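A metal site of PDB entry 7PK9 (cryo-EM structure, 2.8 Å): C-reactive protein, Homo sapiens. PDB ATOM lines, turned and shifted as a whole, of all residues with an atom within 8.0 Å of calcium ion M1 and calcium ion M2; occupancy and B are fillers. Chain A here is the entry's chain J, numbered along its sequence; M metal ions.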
ATOM      1  N   SER A  50      19.011 -19.728  14.001  1.00  0.00           N
ATOM      2  CA  SER A  50      18.588 -18.863  12.900  1.00  0.00           C
ATOM      3  C   SER A  50      17.893 -17.608  13.385  1.00  0.00           C
ATOM      4  O   SER A  50      16.896 -17.680  14.109  1.00  0.00           O
ATOM      5  CB  SER A  50      17.669 -19.617  11.957  1.00  0.00           C
ATOM      6  OG  SER A  50      17.161 -18.725  10.977  1.00  0.00           O
ATOM      7  N   SER A  53      15.565 -16.106   8.082  1.00  0.00           N
ATOM      8  CA  SER A  53      15.685 -17.081   7.005  1.00  0.00           C
ATOM      9  C   SER A  53      14.818 -16.664   5.818  1.00  0.00           C
ATOM     10  O   SER A  53      13.585 -16.653   5.914  1.00  0.00           O
ATOM     11  CB  SER A  53      15.279 -18.463   7.493  1.00  0.00           C
ATOM     12  OG  SER A  53      15.502 -19.449   6.504  1.00  0.00           O
ATOM     13  N   TYR A  54      15.464 -16.317   4.720  1.00  0.00           N
ATOM     14  CA  TYR A  54      14.842 -15.923   3.469  1.00  0.00           C
ATOM     15  C   TYR A  54      15.145 -16.987   2.433  1.00  0.00           C
ATOM     16  O   TYR A  54      16.281 -17.109   1.983  1.00  0.00           O
ATOM     17  CB  TYR A  54      15.380 -14.551   3.056  1.00  0.00           C
ATOM     18  CG  TYR A  54      14.827 -13.923   1.808  1.00  0.00           C
ATOM     19  CD1 TYR A  54      15.089 -14.461   0.563  1.00  0.00           C
ATOM     20  CD2 TYR A  54      14.065 -12.773   1.872  1.00  0.00           C
ATOM     21  CE1 TYR A  54      14.612 -13.869  -0.574  1.00  0.00           C
ATOM     22  CE2 TYR A  54      13.587 -12.177   0.748  1.00  0.00           C
ATOM     23  CZ  TYR A  54      13.860 -12.723  -0.479  1.00  0.00           C
ATOM     24  OH  TYR A  54      13.373 -12.132  -1.616  1.00  0.00           O
ATOM     25  N   ALA A  55      14.142 -17.781   2.063  1.00  0.00           N
ATOM     26  CA  ALA A  55      14.321 -18.891   1.148  1.00  0.00           C
ATOM     27  C   ALA A  55      13.513 -18.685  -0.119  1.00  0.00           C
ATOM     28  O   ALA A  55      12.295 -18.487  -0.051  1.00  0.00           O
ATOM     29  CB  ALA A  55      13.907 -20.210   1.816  1.00  0.00           C
ATOM     30  N   GLN A  59      16.796 -21.741  -3.699  1.00  0.00           N
ATOM     31  CA  GLN A  59      17.856 -21.650  -2.692  1.00  0.00           C
ATOM     32  C   GLN A  59      17.229 -21.394  -1.329  1.00  0.00           C
ATOM     33  O   GLN A  59      16.652 -20.339  -1.103  1.00  0.00           O
ATOM     34  CB  GLN A  59      18.847 -20.557  -3.045  1.00  0.00           C
ATOM     35  CG  GLN A  59      20.004 -20.443  -2.078  1.00  0.00           C
ATOM     36  CD  GLN A  59      20.896 -21.654  -2.081  1.00  0.00           C
ATOM     37  OE1 GLN A  59      21.201 -22.212  -3.126  1.00  0.00           O
ATOM     38  NE2 GLN A  59      21.301 -22.084  -0.901  1.00  0.00           N
ATOM     39  N   ASP A  60      17.346 -22.379  -0.425  1.00  0.00           N
ATOM     40  CA  ASP A  60      16.778 -22.259   0.908  1.00  0.00           C
ATOM     41  C   ASP A  60      17.533 -21.264   1.785  1.00  0.00           C
ATOM     42  O   ASP A  60      16.964 -20.777   2.766  1.00  0.00           O
ATOM     43  CB  ASP A  60      16.784 -23.624   1.600  1.00  0.00           C
ATOM     44  CG  ASP A  60      18.184 -24.191   1.758  1.00  0.00           C
ATOM     45  OD1 ASP A  60      18.837 -24.485   0.734  1.00  0.00           O
ATOM     46  OD2 ASP A  60      18.632 -24.349   2.907  1.00  0.00           O
ATOM     47  N   ASN A  61      18.794 -20.969   1.461  1.00  0.00           N
ATOM     48  CA  ASN A  61      19.571 -19.992   2.203  1.00  0.00           C
ATOM     49  C   ASN A  61      19.824 -18.755   1.346  1.00  0.00           C
ATOM     50  O   ASN A  61      20.971 -18.365   1.137  1.00  0.00           O
ATOM     51  CB  ASN A  61      20.894 -20.583   2.669  1.00  0.00           C
ATOM     52  CG  ASN A  61      20.707 -21.710   3.657  1.00  0.00           C
ATOM     53  OD1 ASN A  61      19.595 -21.982   4.106  1.00  0.00           O
ATOM     54  ND2 ASN A  61      21.805 -22.356   4.021  1.00  0.00           N
ATOM     55  N   GLU A  62      18.754 -18.173   0.812  1.00  0.00           N
ATOM     56  CA  GLU A  62      18.903 -17.062  -0.114  1.00  0.00           C
ATOM     57  C   GLU A  62      19.314 -15.769   0.604  1.00  0.00           C
ATOM     58  O   GLU A  62      20.162 -15.039   0.107  1.00  0.00           O
ATOM     59  CB  GLU A  62      17.594 -16.875  -0.869  1.00  0.00           C
ATOM     60  CG  GLU A  62      17.603 -15.777  -1.892  1.00  0.00           C
ATOM     61  CD  GLU A  62      18.539 -16.076  -3.029  1.00  0.00           C
ATOM     62  OE1 GLU A  62      18.800 -17.254  -3.297  1.00  0.00           O
ATOM     63  OE2 GLU A  62      19.012 -15.115  -3.650  1.00  0.00           O
ATOM     64  N   LEU A  64      20.405 -15.469   4.764  1.00  0.00           N
ATOM     65  CA  LEU A  64      20.405 -16.039   6.105  1.00  0.00           C
ATOM     66  C   LEU A  64      21.355 -15.289   6.998  1.00  0.00           C
ATOM     67  O   LEU A  64      22.537 -15.154   6.677  1.00  0.00           O
ATOM     68  CB  LEU A  64      20.787 -17.512   6.059  1.00  0.00           C
ATOM     69  CG  LEU A  64      20.551 -18.271   7.354  1.00  0.00           C
ATOM     70  CD1 LEU A  64      19.095 -18.318   7.718  1.00  0.00           C
ATOM     71  CD2 LEU A  64      21.104 -19.665   7.224  1.00  0.00           C
ATOM     72  N   PHE A  66      22.750 -15.900  10.631  1.00  0.00           N
ATOM     73  CA  PHE A  66      22.826 -17.030  11.541  1.00  0.00           C
ATOM     74  C   PHE A  66      23.879 -16.738  12.597  1.00  0.00           C
ATOM     75  O   PHE A  66      25.037 -16.506  12.259  1.00  0.00           O
ATOM     76  CB  PHE A  66      23.140 -18.314  10.775  1.00  0.00           C
ATOM     77  CG  PHE A  66      22.808 -19.568  11.516  1.00  0.00           C
ATOM     78  CD1 PHE A  66      21.550 -20.113  11.450  1.00  0.00           C
ATOM     79  CD2 PHE A  66      23.788 -20.228  12.220  1.00  0.00           C
ATOM     80  CE1 PHE A  66      21.266 -21.279  12.120  1.00  0.00           C
ATOM     81  CE2 PHE A  66      23.503 -21.381  12.886  1.00  0.00           C
ATOM     82  CZ  PHE A  66      22.244 -21.921  12.833  1.00  0.00           C
ATOM     83  N   THR A  76      24.841 -14.915   5.042  1.00  0.00           N
ATOM     84  CA  THR A  76      24.922 -15.608   3.763  1.00  0.00           C
ATOM     85  C   THR A  76      23.890 -15.089   2.776  1.00  0.00           C
ATOM     86  O   THR A  76      22.737 -14.842   3.134  1.00  0.00           O
ATOM     87  CB  THR A  76      24.694 -17.113   3.904  1.00  0.00           C
ATOM     88  OG1 THR A  76      23.296 -17.376   3.938  1.00  0.00           O
ATOM     89  CG2 THR A  76      25.281 -17.624   5.176  1.00  0.00           C
ATOM     90  N   GLN A 137      12.752 -19.960  12.861  1.00  0.00           N
ATOM     91  CA  GLN A 137      13.239 -21.244  12.398  1.00  0.00           C
ATOM     92  C   GLN A 137      14.276 -21.029  11.305  1.00  0.00           C
ATOM     93  O   GLN A 137      14.392 -19.964  10.719  1.00  0.00           O
ATOM     94  CB  GLN A 137      12.117 -22.132  11.852  1.00  0.00           C
ATOM     95  CG  GLN A 137      11.069 -22.495  12.857  1.00  0.00           C
ATOM     96  CD  GLN A 137      11.600 -23.404  13.939  1.00  0.00           C
ATOM     97  OE1 GLN A 137      12.626 -24.051  13.766  1.00  0.00           O
ATOM     98  NE2 GLN A 137      10.903 -23.451  15.060  1.00  0.00           N
ATOM     99  N   GLU A 138      15.017 -22.102  11.046  1.00  0.00           N
ATOM    100  CA  GLU A 138      15.860 -22.237   9.877  1.00  0.00           C
ATOM    101  C   GLU A 138      15.180 -23.188   8.915  1.00  0.00           C
ATOM    102  O   GLU A 138      14.829 -24.308   9.287  1.00  0.00           O
ATOM    103  CB  GLU A 138      17.228 -22.789  10.258  1.00  0.00           C
ATOM    104  CG  GLU A 138      18.174 -22.937   9.097  1.00  0.00           C
ATOM    105  CD  GLU A 138      18.520 -21.633   8.505  1.00  0.00           C
ATOM    106  OE1 GLU A 138      18.448 -20.650   9.256  1.00  0.00           O
ATOM    107  OE2 GLU A 138      18.864 -21.592   7.305  1.00  0.00           O
ATOM    108  N   GLN A 139      15.015 -22.742   7.680  1.00  0.00           N
ATOM    109  CA  GLN A 139      14.355 -23.549   6.668  1.00  0.00           C
ATOM    110  C   GLN A 139      15.399 -24.048   5.679  1.00  0.00           C
ATOM    111  O   GLN A 139      16.189 -23.259   5.161  1.00  0.00           O
ATOM    112  CB  GLN A 139      13.237 -22.760   6.007  1.00  0.00           C
ATOM    113  CG  GLN A 139      13.637 -21.722   5.026  1.00  0.00           C
ATOM    114  CD  GLN A 139      12.583 -20.649   4.902  1.00  0.00           C
ATOM    115  OE1 GLN A 139      11.540 -20.861   4.304  1.00  0.00           O
ATOM    116  NE2 GLN A 139      12.869 -19.482   5.439  1.00  0.00           N
ATOM    117  N   ASP A 140      15.405 -25.357   5.442  1.00  0.00           N
ATOM    118  CA  ASP A 140      16.298 -26.004   4.500  1.00  0.00           C
ATOM    119  C   ASP A 140      15.602 -26.396   3.209  1.00  0.00           C
ATOM    120  O   ASP A 140      16.272 -26.816   2.255  1.00  0.00           O
ATOM    121  CB  ASP A 140      16.915 -27.254   5.151  1.00  0.00           C
ATOM    122  CG  ASP A 140      17.981 -26.915   6.163  1.00  0.00           C
ATOM    123  OD1 ASP A 140      18.089 -27.609   7.183  1.00  0.00           O
ATOM    124  OD2 ASP A 140      18.735 -25.933   5.939  1.00  0.00           O
ATOM    125  N   SER A 141      14.283 -26.272   3.155  1.00  0.00           N
ATOM    126  CA  SER A 141      13.522 -26.345   1.932  1.00  0.00           C
ATOM    127  C   SER A 141      12.592 -25.145   1.922  1.00  0.00           C
ATOM    128  O   SER A 141      12.394 -24.486   2.954  1.00  0.00           O
ATOM    129  CB  SER A 141      12.731 -27.651   1.811  1.00  0.00           C
ATOM    130  OG  SER A 141      11.707 -27.749   2.771  1.00  0.00           O
ATOM    131  N   GLY A 144      10.090 -24.949   4.778  1.00  0.00           N
ATOM    132  CA  GLY A 144       9.976 -26.170   5.554  1.00  0.00           C
ATOM    133  C   GLY A 144      11.317 -26.748   5.935  1.00  0.00           C
ATOM    134  O   GLY A 144      12.360 -26.108   5.807  1.00  0.00           O
ATOM    135  N   ASN A 145      11.255 -27.985   6.428  1.00  0.00           N
ATOM    136  CA  ASN A 145      12.433 -28.700   6.920  1.00  0.00           C
ATOM    137  C   ASN A 145      13.138 -27.924   8.026  1.00  0.00           C
ATOM    138  O   ASN A 145      14.362 -27.720   7.996  1.00  0.00           O
ATOM    139  CB  ASN A 145      13.393 -29.027   5.778  1.00  0.00           C
ATOM    140  CG  ASN A 145      12.790 -29.953   4.768  1.00  0.00           C
ATOM    141  OD1 ASN A 145      11.618 -30.313   4.870  1.00  0.00           O
ATOM    142  ND2 ASN A 145      13.582 -30.379   3.790  1.00  0.00           N
ATOM    143  N   PHE A 146      12.362 -27.469   8.995  1.00  0.00           N
ATOM    144  CA  PHE A 146      12.919 -26.795  10.149  1.00  0.00           C
ATOM    145  C   PHE A 146      13.681 -27.773  11.031  1.00  0.00           C
ATOM    146  O   PHE A 146      13.411 -28.979  11.048  1.00  0.00           O
ATOM    147  CB  PHE A 146      11.811 -26.125  10.948  1.00  0.00           C
ATOM    148  CG  PHE A 146      10.933 -25.255  10.109  1.00  0.00           C
ATOM    149  CD1 PHE A 146      11.465 -24.287   9.295  1.00  0.00           C
ATOM    150  CD2 PHE A 146       9.560 -25.402  10.145  1.00  0.00           C
ATOM    151  CE1 PHE A 146      10.658 -23.486   8.539  1.00  0.00           C
ATOM    152  CE2 PHE A 146       8.754 -24.609   9.384  1.00  0.00           C
ATOM    153  CZ  PHE A 146       9.307 -23.643   8.579  1.00  0.00           C
ATOM    154  N   GLU A 147      14.659 -27.233  11.769  1.00  0.00           N
ATOM    155  CA  GLU A 147      15.411 -27.997  12.763  1.00  0.00           C
ATOM    156  C   GLU A 147      15.354 -27.256  14.087  1.00  0.00           C
ATOM    157  O   GLU A 147      15.710 -26.085  14.159  1.00  0.00           O
ATOM    158  CB  GLU A 147      16.861 -28.202  12.314  1.00  0.00           C
ATOM    159  CG  GLU A 147      16.996 -28.850  10.943  1.00  0.00           C
ATOM    160  CD  GLU A 147      18.425 -29.272  10.620  1.00  0.00           C
ATOM    161  OE1 GLU A 147      19.090 -28.608   9.809  1.00  0.00           O
ATOM    162  OE2 GLU A 147      18.877 -30.282  11.204  1.00  0.00           O
ATOM    163  N   GLY A 148      14.918 -27.957  15.133  1.00  0.00           N
ATOM    164  CA  GLY A 148      14.785 -27.330  16.437  1.00  0.00           C
ATOM    165  C   GLY A 148      16.094 -26.773  16.967  1.00  0.00           C
ATOM    166  O   GLY A 148      16.129 -25.691  17.558  1.00  0.00           O
ATOM    167  N   SER A 149      17.191 -27.501  16.771  1.00  0.00           N
ATOM    168  CA  SER A 149      18.502 -27.041  17.183  1.00  0.00           C
ATOM    169  C   SER A 149      18.942 -25.763  16.470  1.00  0.00           C
ATOM    170  O   SER A 149      20.023 -25.250  16.746  1.00  0.00           O
ATOM    171  CB  SER A 149      19.540 -28.146  16.953  1.00  0.00           C
ATOM    172  OG  SER A 149      19.705 -28.419  15.570  1.00  0.00           O
ATOM    173  N   GLN A 150      18.135 -25.265  15.534  1.00  0.00           N
ATOM    174  CA  GLN A 150      18.371 -23.975  14.897  1.00  0.00           C
ATOM    175  C   GLN A 150      17.254 -22.958  15.122  1.00  0.00           C
ATOM    176  O   GLN A 150      17.353 -21.838  14.622  1.00  0.00           O
ATOM    177  CB  GLN A 150      18.581 -24.209  13.407  1.00  0.00           C
ATOM    178  CG  GLN A 150      19.831 -25.018  13.146  1.00  0.00           C
ATOM    179  CD  GLN A 150      20.221 -25.097  11.689  1.00  0.00           C
ATOM    180  OE1 GLN A 150      19.368 -25.152  10.820  1.00  0.00           O
ATOM    181  NE2 GLN A 150      21.515 -25.119  11.436  1.00  0.00           N
HETATM  182 CA    CA M   1      18.960 -26.270   8.839  1.00  0.00          CA
HETATM  183 CA    CA M   2      18.984 -23.772   5.424  1.00  0.00          CA
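Four residues have an atom within 4 Å of calcium ion M1: Glu 138, Asp 140, Glu 147 and Gln 150.
Within 4 Å of calcium ion M2: Asp 60, Asn 61, Glu 138, Gln 139 and Asp 140.
The backbone carbonyl oxygen of Gln 150 lies within hydrogen-bond range of the backbone NH of Ser 50, 2.8 Å away. NE2 of Gln 139 lies within hydrogen-bond range of OG of Ser 53 (2.8 Å). The side-chain hydroxyl of Ser 50 is in hydrogen-bond range of the side-chain carboxylate of Glu 138, 2.9 Å away.
Calcium ion M2 is bound by the side-chain carboxylate of Asp 140 (2.2 Å), the side-chain amide oxygen of Asn 61 (2.3 Å), the side-chain carboxylate of Asp 60 (2.6 Å), the backbone carbonyl oxygen of Gln 139 (2.9 Å) and the side-chain carboxylate of Glu 138 (2.9 Å).
Calcium ion M1 is bound by OD1 of Asp 140 (2.3 Å), OE1 of Gln 150 (2.3 Å) and OE1 of Glu 147 (2.5 Å). Slightly farther from calcium ion M1 lies the side-chain carboxylate (OD2) of Asp 140 (2.9 Å).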
